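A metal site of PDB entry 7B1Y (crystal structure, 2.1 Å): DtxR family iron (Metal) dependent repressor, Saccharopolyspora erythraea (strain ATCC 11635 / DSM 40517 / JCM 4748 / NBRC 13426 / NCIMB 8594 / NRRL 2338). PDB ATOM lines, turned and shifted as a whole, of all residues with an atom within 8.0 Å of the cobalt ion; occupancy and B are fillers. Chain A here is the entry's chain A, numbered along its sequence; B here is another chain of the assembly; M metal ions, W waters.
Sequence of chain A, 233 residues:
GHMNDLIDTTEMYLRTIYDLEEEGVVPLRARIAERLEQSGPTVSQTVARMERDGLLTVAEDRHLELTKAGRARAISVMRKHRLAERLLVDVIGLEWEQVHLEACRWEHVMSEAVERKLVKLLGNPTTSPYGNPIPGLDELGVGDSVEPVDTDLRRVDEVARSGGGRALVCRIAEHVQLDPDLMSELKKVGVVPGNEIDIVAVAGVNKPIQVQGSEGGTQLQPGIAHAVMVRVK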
ATOM      1  N   ARG A  15       9.734  36.606   7.619  1.00  0.00           N
ATOM      2  CA  ARG A  15       9.217  35.309   7.111  1.00  0.00           C
ATOM      3  C   ARG A  15      10.379  34.487   6.530  1.00  0.00           C
ATOM      4  O   ARG A  15      10.356  33.257   6.699  1.00  0.00           O
ATOM      5  CB  ARG A  15       8.101  35.507   6.064  1.00  0.00           C
ATOM      6  CG  ARG A  15       7.047  34.419   6.082  1.00  0.00           C
ATOM      7  CD  ARG A  15       6.449  34.172   4.714  1.00  0.00           C
ATOM      8  NE  ARG A  15       7.327  33.377   3.876  1.00  0.00           N
ATOM      9  CZ  ARG A  15       7.312  33.333   2.551  1.00  0.00           C
ATOM     10  NH1 ARG A  15       6.434  34.048   1.855  1.00  0.00           N
ATOM     11  NH2 ARG A  15       8.176  32.562   1.903  1.00  0.00           N
ATOM     12  N   ASP A  19      11.450  30.853   7.617  1.00  0.00           N
ATOM     13  CA  ASP A  19      11.634  29.802   6.587  1.00  0.00           C
ATOM     14  C   ASP A  19      12.912  29.009   6.883  1.00  0.00           C
ATOM     15  O   ASP A  19      12.848  27.766   6.905  1.00  0.00           O
ATOM     16  CB  ASP A  19      11.712  30.389   5.170  1.00  0.00           C
ATOM     17  CG  ASP A  19      10.408  30.971   4.641  1.00  0.00           C
ATOM     18  OD1 ASP A  19       9.362  30.747   5.274  1.00  0.00           O
ATOM     19  OD2 ASP A  19      10.456  31.649   3.595  1.00  0.00           O
ATOM     20  N   MET A  78       3.055  34.333   8.325  1.00  0.00           N
ATOM     21  CA  MET A  78       3.074  32.918   7.859  1.00  0.00           C
ATOM     22  C   MET A  78       1.669  32.329   7.934  1.00  0.00           C
ATOM     23  O   MET A  78       1.280  31.586   7.011  1.00  0.00           O
ATOM     24  CB  MET A  78       4.036  32.065   8.698  1.00  0.00           C
ATOM     25  CG  MET A  78       4.233  30.659   8.166  1.00  0.00           C
ATOM     26  SD  MET A  78       4.958  30.636   6.502  1.00  0.00           S
ATOM     27  CE  MET A  78       6.673  30.895   6.906  1.00  0.00           C
ATOM     28  N   HIS A  81      -0.288  33.778   5.104  1.00  0.00           N
ATOM     29  CA  HIS A  81       0.280  33.104   3.904  1.00  0.00           C
ATOM     30  C   HIS A  81      -0.423  31.764   3.661  1.00  0.00           C
ATOM     31  O   HIS A  81      -0.959  31.563   2.546  1.00  0.00           O
ATOM     32  CB  HIS A  81       1.792  32.933   4.054  1.00  0.00           C
ATOM     33  CG  HIS A  81       2.443  32.281   2.882  1.00  0.00           C
ATOM     34  ND1 HIS A  81       2.799  32.995   1.767  1.00  0.00           N
ATOM     35  CD2 HIS A  81       2.762  30.993   2.648  1.00  0.00           C
ATOM     36  CE1 HIS A  81       3.336  32.163   0.886  1.00  0.00           C
ATOM     37  NE2 HIS A  81       3.321  30.938   1.403  1.00  0.00           N
ATOM     38  N   ARG A  82      -0.443  30.890   4.665  1.00  0.00           N
ATOM     39  CA  ARG A  82      -0.860  29.463   4.524  1.00  0.00           C
ATOM     40  C   ARG A  82      -2.382  29.357   4.464  1.00  0.00           C
ATOM     41  O   ARG A  82      -2.875  28.414   3.810  1.00  0.00           O
ATOM     42  CB  ARG A  82      -0.217  28.628   5.632  1.00  0.00           C
ATOM     43  CG  ARG A  82       1.274  28.421   5.411  1.00  0.00           C
ATOM     44  CD  ARG A  82       2.047  27.699   6.500  1.00  0.00           C
ATOM     45  NE  ARG A  82       3.440  27.627   6.091  1.00  0.00           N
ATOM     46  CZ  ARG A  82       4.469  27.299   6.868  1.00  0.00           C
ATOM     47  NH1 ARG A  82       4.293  26.985   8.145  1.00  0.00           N
ATOM     48  NH2 ARG A  82       5.693  27.279   6.356  1.00  0.00           N
ATOM     49  N   GLU A  85      -3.172  30.348   0.845  1.00  0.00           N
ATOM     50  CA  GLU A  85      -2.839  29.183  -0.030  1.00  0.00           C
ATOM     51  C   GLU A  85      -4.029  28.208  -0.049  1.00  0.00           C
ATOM     52  O   GLU A  85      -4.392  27.756  -1.150  1.00  0.00           O
ATOM     53  CB  GLU A  85      -1.572  28.487   0.457  1.00  0.00           C
ATOM     54  CG  GLU A  85      -0.309  29.266   0.158  1.00  0.00           C
ATOM     55  CD  GLU A  85       0.979  28.596   0.607  1.00  0.00           C
ATOM     56  OE1 GLU A  85       0.950  27.887   1.624  1.00  0.00           O
ATOM     57  OE2 GLU A  85       2.004  28.781  -0.073  1.00  0.00           O
ATOM     58  N   VAL A  99       0.261  29.119  -6.732  1.00  0.00           N
ATOM     59  CA  VAL A  99      -0.496  29.503  -5.504  1.00  0.00           C
ATOM     60  C   VAL A  99       0.422  30.283  -4.544  1.00  0.00           C
ATOM     61  O   VAL A  99      -0.004  31.347  -4.060  1.00  0.00           O
ATOM     62  CB  VAL A  99      -1.136  28.277  -4.825  1.00  0.00           C
ATOM     63  CG1 VAL A  99      -1.408  28.506  -3.344  1.00  0.00           C
ATOM     64  CG2 VAL A  99      -2.409  27.863  -5.546  1.00  0.00           C
ATOM     65  N   HIS A 100       1.621  29.748  -4.267  1.00  0.00           N
ATOM     66  CA  HIS A 100       2.589  30.336  -3.289  1.00  0.00           C
ATOM     67  C   HIS A 100       2.938  31.766  -3.685  1.00  0.00           C
ATOM     68  O   HIS A 100       2.915  32.643  -2.793  1.00  0.00           O
ATOM     69  CB  HIS A 100       3.832  29.446  -3.161  1.00  0.00           C
ATOM     70  CG  HIS A 100       4.931  30.104  -2.396  1.00  0.00           C
ATOM     71  ND1 HIS A 100       4.971  30.107  -1.018  1.00  0.00           N
ATOM     72  CD2 HIS A 100       6.009  30.799  -2.812  1.00  0.00           C
ATOM     73  CE1 HIS A 100       6.036  30.772  -0.613  1.00  0.00           C
ATOM     74  NE2 HIS A 100       6.688  31.196  -1.692  1.00  0.00           N
ATOM     75  N   LEU A 101       3.252  32.005  -4.961  1.00  0.00           N
ATOM     76  CA  LEU A 101       3.656  33.333  -5.513  1.00  0.00           C
ATOM     77  C   LEU A 101       2.526  34.346  -5.280  1.00  0.00           C
ATOM     78  O   LEU A 101       2.835  35.526  -5.043  1.00  0.00           O
ATOM     79  CB  LEU A 101       3.971  33.210  -7.007  1.00  0.00           C
ATOM     80  CG  LEU A 101       5.406  32.785  -7.349  1.00  0.00           C
ATOM     81  CD1 LEU A 101       5.647  31.323  -6.998  1.00  0.00           C
ATOM     82  CD2 LEU A 101       5.700  33.030  -8.817  1.00  0.00           C
ATOM     83  N   ALA A 103       0.041  33.961  -2.763  1.00  0.00           N
ATOM     84  CA  ALA A 103      -0.059  34.017  -1.288  1.00  0.00           C
ATOM     85  C   ALA A 103       1.102  34.824  -0.715  1.00  0.00           C
ATOM     86  O   ALA A 103       1.002  35.347   0.396  1.00  0.00           O
ATOM     87  CB  ALA A 103      -0.105  32.631  -0.718  1.00  0.00           C
ATOM     88  N   CSD A 104       2.209  34.908  -1.454  1.00  0.00           N
ATOM     89  CA  CSD A 104       3.391  35.650  -1.034  1.00  0.00           C
ATOM     90  CB  CSD A 104       4.589  35.351  -1.941  1.00  0.00           C
ATOM     91  SG  CSD A 104       6.102  35.340  -0.943  1.00  0.00           S
ATOM     92  C   CSD A 104       3.100  37.157  -1.016  1.00  0.00           C
ATOM     93  O   CSD A 104       3.759  37.894  -0.305  1.00  0.00           O
ATOM     94  OD1 CSD A 104       7.082  34.507  -1.689  1.00  0.00           O
ATOM     95  OD2 CSD A 104       6.669  36.833  -0.875  1.00  0.00           O
ATOM     96  N   GLU A 107      -0.289  37.711   1.840  1.00  0.00           N
ATOM     97  CA  GLU A 107       0.119  37.585   3.265  1.00  0.00           C
ATOM     98  C   GLU A 107       0.320  38.962   3.923  1.00  0.00           C
ATOM     99  O   GLU A 107       0.282  39.028   5.158  1.00  0.00           O
ATOM    100  CB  GLU A 107       1.389  36.734   3.404  1.00  0.00           C
ATOM    101  CG  GLU A 107       2.619  37.338   2.755  1.00  0.00           C
ATOM    102  CD  GLU A 107       3.860  36.454   2.773  1.00  0.00           C
ATOM    103  OE1 GLU A 107       3.788  35.344   3.342  1.00  0.00           O
ATOM    104  OE2 GLU A 107       4.900  36.869   2.235  1.00  0.00           O
ATOM    105  N   SER A 128      -1.160  23.921   5.444  1.00  0.00           N
ATOM    106  CA  SER A 128      -1.267  24.500   4.079  1.00  0.00           C
ATOM    107  C   SER A 128      -1.416  23.352   3.068  1.00  0.00           C
ATOM    108  O   SER A 128      -1.239  22.193   3.438  1.00  0.00           O
ATOM    109  CB  SER A 128      -0.078  25.368   3.769  1.00  0.00           C
ATOM    110  OG  SER A 128       1.056  24.579   3.418  1.00  0.00           O
ATOM    111  N   PRO A 129      -1.722  23.629   1.782  1.00  0.00           N
ATOM    112  CA  PRO A 129      -1.807  22.582   0.762  1.00  0.00           C
ATOM    113  C   PRO A 129      -0.499  21.829   0.527  1.00  0.00           C
ATOM    114  O   PRO A 129      -0.529  20.788  -0.119  1.00  0.00           O
ATOM    115  CB  PRO A 129      -2.215  23.324  -0.518  1.00  0.00           C
ATOM    116  CG  PRO A 129      -2.781  24.653  -0.039  1.00  0.00           C
ATOM    117  CD  PRO A 129      -2.009  24.970   1.230  1.00  0.00           C
ATOM    118  N   TYR A 130       0.627  22.361   1.020  1.00  0.00           N
ATOM    119  CA  TYR A 130       1.990  21.782   0.863  1.00  0.00           C
ATOM    120  C   TYR A 130       2.430  21.110   2.163  1.00  0.00           C
ATOM    121  O   TYR A 130       3.625  20.795   2.292  1.00  0.00           O
ATOM    122  CB  TYR A 130       2.952  22.887   0.411  1.00  0.00           C
ATOM    123  CG  TYR A 130       2.414  23.709  -0.725  1.00  0.00           C
ATOM    124  CD1 TYR A 130       2.298  23.167  -2.003  1.00  0.00           C
ATOM    125  CD2 TYR A 130       1.957  25.001  -0.530  1.00  0.00           C
ATOM    126  CE1 TYR A 130       1.781  23.909  -3.050  1.00  0.00           C
ATOM    127  CE2 TYR A 130       1.441  25.751  -1.571  1.00  0.00           C
ATOM    128  CZ  TYR A 130       1.355  25.210  -2.839  1.00  0.00           C
ATOM    129  OH  TYR A 130       0.843  25.939  -3.869  1.00  0.00           O
ATOM    130  N   ASN A 132       2.643  22.132   5.264  1.00  0.00           N
ATOM    131  CA  ASN A 132       3.317  22.977   6.283  1.00  0.00           C
ATOM    132  C   ASN A 132       2.285  23.391   7.335  1.00  0.00           C
ATOM    133  O   ASN A 132       1.244  23.939   6.988  1.00  0.00           O
ATOM    134  CB  ASN A 132       3.989  24.197   5.660  1.00  0.00           C
ATOM    135  CG  ASN A 132       5.027  23.821   4.625  1.00  0.00           C
ATOM    136  OD1 ASN A 132       5.875  22.966   4.871  1.00  0.00           O
ATOM    137  ND2 ASN A 132       4.969  24.447   3.459  1.00  0.00           N
ATOM    138  N   ILE B 172       6.436  20.260   2.052  1.00  0.00           N
ATOM    139  CA  ILE B 172       7.297  20.929   1.021  1.00  0.00           C
ATOM    140  C   ILE B 172       7.476  22.390   1.467  1.00  0.00           C
ATOM    141  O   ILE B 172       6.492  23.151   1.364  1.00  0.00           O
ATOM    142  CB  ILE B 172       6.678  20.807  -0.379  1.00  0.00           C
ATOM    143  CG1 ILE B 172       6.474  19.350  -0.792  1.00  0.00           C
ATOM    144  CG2 ILE B 172       7.515  21.571  -1.400  1.00  0.00           C
ATOM    145  CD1 ILE B 172       5.707  19.154  -2.074  1.00  0.00           C
ATOM    146  N   ALA B 173       8.672  22.742   1.943  1.00  0.00           N
ATOM    147  CA  ALA B 173       8.986  24.069   2.537  1.00  0.00           C
ATOM    148  C   ALA B 173       8.790  25.180   1.508  1.00  0.00           C
ATOM    149  O   ALA B 173       8.742  24.867   0.299  1.00  0.00           O
ATOM    150  CB  ALA B 173      10.398  24.066   3.080  1.00  0.00           C
ATOM    151  N   GLU B 174       8.703  26.428   1.987  1.00  0.00           N
ATOM    152  CA  GLU B 174       8.368  27.642   1.191  1.00  0.00           C
ATOM    153  C   GLU B 174       9.447  27.888   0.116  1.00  0.00           C
ATOM    154  O   GLU B 174       9.098  28.428  -0.947  1.00  0.00           O
ATOM    155  CB  GLU B 174       8.230  28.869   2.094  1.00  0.00           C
ATOM    156  CG  GLU B 174       7.213  28.718   3.218  1.00  0.00           C
ATOM    157  CD  GLU B 174       5.774  28.482   2.800  1.00  0.00           C
ATOM    158  OE1 GLU B 174       4.991  27.995   3.643  1.00  0.00           O
ATOM    159  OE2 GLU B 174       5.421  28.782   1.641  1.00  0.00           O
ATOM    160  N   HIS B 175      10.701  27.525   0.407  1.00  0.00           N
ATOM    161  CA  HIS B 175      11.867  27.674  -0.496  1.00  0.00           C
ATOM    162  C   HIS B 175      11.642  26.882  -1.795  1.00  0.00           C
ATOM    163  O   HIS B 175      11.993  27.406  -2.870  1.00  0.00           O
ATOM    164  CB  HIS B 175      13.155  27.256   0.220  1.00  0.00           C
ATOM    165  CG  HIS B 175      14.364  27.230  -0.653  1.00  0.00           C
ATOM    166  ND1 HIS B 175      14.826  28.352  -1.321  1.00  0.00           N
ATOM    167  CD2 HIS B 175      15.226  26.226  -0.950  1.00  0.00           C
ATOM    168  CE1 HIS B 175      15.904  28.040  -2.009  1.00  0.00           C
ATOM    169  NE2 HIS B 175      16.171  26.741  -1.799  1.00  0.00           N
ATOM    170  N   VAL B 176      11.076  25.680  -1.683  1.00  0.00           N
ATOM    171  CA  VAL B 176      10.800  24.761  -2.835  1.00  0.00           C
ATOM    172  C   VAL B 176       9.702  25.376  -3.707  1.00  0.00           C
ATOM    173  O   VAL B 176       9.791  25.255  -4.941  1.00  0.00           O
ATOM    174  CB  VAL B 176      10.403  23.353  -2.363  1.00  0.00           C
ATOM    175  CG1 VAL B 176      10.196  22.401  -3.530  1.00  0.00           C
ATOM    176  CG2 VAL B 176      11.409  22.775  -1.378  1.00  0.00           C
ATOM    177  N   GLN B 177       8.715  26.033  -3.076  1.00  0.00           N
ATOM    178  CA  GLN B 177       7.491  26.555  -3.737  1.00  0.00           C
ATOM    179  C   GLN B 177       7.830  27.761  -4.623  1.00  0.00           C
ATOM    180  O   GLN B 177       7.022  28.055  -5.533  1.00  0.00           O
ATOM    181  CB  GLN B 177       6.451  26.934  -2.688  1.00  0.00           C
ATOM    182  CG  GLN B 177       6.019  25.779  -1.794  1.00  0.00           C
ATOM    183  CD  GLN B 177       5.125  26.224  -0.666  1.00  0.00           C
ATOM    184  OE1 GLN B 177       4.383  27.190  -0.789  1.00  0.00           O
ATOM    185  NE2 GLN B 177       5.182  25.510   0.450  1.00  0.00           N
ATOM    186  N   LEU B 178       8.963  28.430  -4.384  1.00  0.00           N
ATOM    187  CA  LEU B 178       9.395  29.660  -5.111  1.00  0.00           C
ATOM    188  C   LEU B 178       9.669  29.351  -6.585  1.00  0.00           C
ATOM    189  O   LEU B 178       9.505  30.272  -7.410  1.00  0.00           O
ATOM    190  CB  LEU B 178      10.633  30.265  -4.443  1.00  0.00           C
ATOM    191  CG  LEU B 178      10.389  31.472  -3.549  1.00  0.00           C
ATOM    192  CD1 LEU B 178      11.664  31.892  -2.836  1.00  0.00           C
ATOM    193  CD2 LEU B 178       9.827  32.642  -4.344  1.00  0.00           C
ATOM    194  N   MET B 183       7.901  22.764  -9.090  1.00  0.00           N
ATOM    195  CA  MET B 183       6.635  22.345  -8.434  1.00  0.00           C
ATOM    196  C   MET B 183       5.767  21.577  -9.433  1.00  0.00           C
ATOM    197  O   MET B 183       5.143  20.580  -9.017  1.00  0.00           O
ATOM    198  CB  MET B 183       5.861  23.563  -7.897  1.00  0.00           C
ATOM    199  CG  MET B 183       6.499  24.189  -6.677  1.00  0.00           C
ATOM    200  SD  MET B 183       6.516  23.093  -5.225  1.00  0.00           S
ATOM    201  CE  MET B 183       4.820  23.256  -4.681  1.00  0.00           C
HETATM  202 CO    CO M   1       3.946  29.017   0.435  1.00  0.00          CO
HETATM  203  O   HOH W   1       3.029  26.740   2.457  1.00  0.00           O
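Water W1 lies within hydrogen-bond range of OE1 of Glu 85 (2.5 Å), OE1 of Glu 174 of chain B (2.6 Å), OG of Ser 128 (3.1 Å), ND2 of Asn 132 (3.2 Å) and NE2 of Gln 177 of chain B (3.2 Å).
Five residues have an atom within 4 Å of the cobalt ion: His 81, Glu 85, His 100, Glu 174 of chain B and Gln 177 of chain B.
The cobalt ion is bound by OE2 of Glu 174 of chain B, at 1.9 Å.
OE2 of Glu 85 binds the cobalt ion (2.0 Å).
The cobalt ion is bound by ND1 of His 100 (2.1 Å).
NE2 of His 81 is bound to the cobalt ion (2.2 Å).
OE1 of Gln 177 of chain B is bound to the cobalt ion (2.2 Å).
The cobalt ion has five donor atoms within binding distance.
The guanidinium group (NH2) of Arg 82 is in salt-bridge range of the side-chain carboxylate (OE1) of Glu 174 of chain B, 2.9 Å away.
A ring nitrogen (NE2) of His 100 lies within hydrogen-bond range of OD1 of CSD 104 (3.3 Å).
A ring nitrogen (ND1) of His 81 is in hydrogen-bond range of the backbone carbonyl oxygen (O) of Ala 103 (3.3 Å).
A ring nitrogen (ND1) of His 81 sits at hydrogen-bond distance from the side-chain carboxylate (OE1) of Glu 107, at 3.0 Å.
The side-chain amide nitrogen (NE2) of Gln 177 of chain B sits close to the side-chain amide nitrogen (ND2) of Asn 132, 3.2 Å away.
The backbone carbonyl oxygen of Ile 172 of chain B sits at hydrogen-bond distance from the side-chain amide nitrogen of Gln 177 of chain B, at 2.8 Å.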
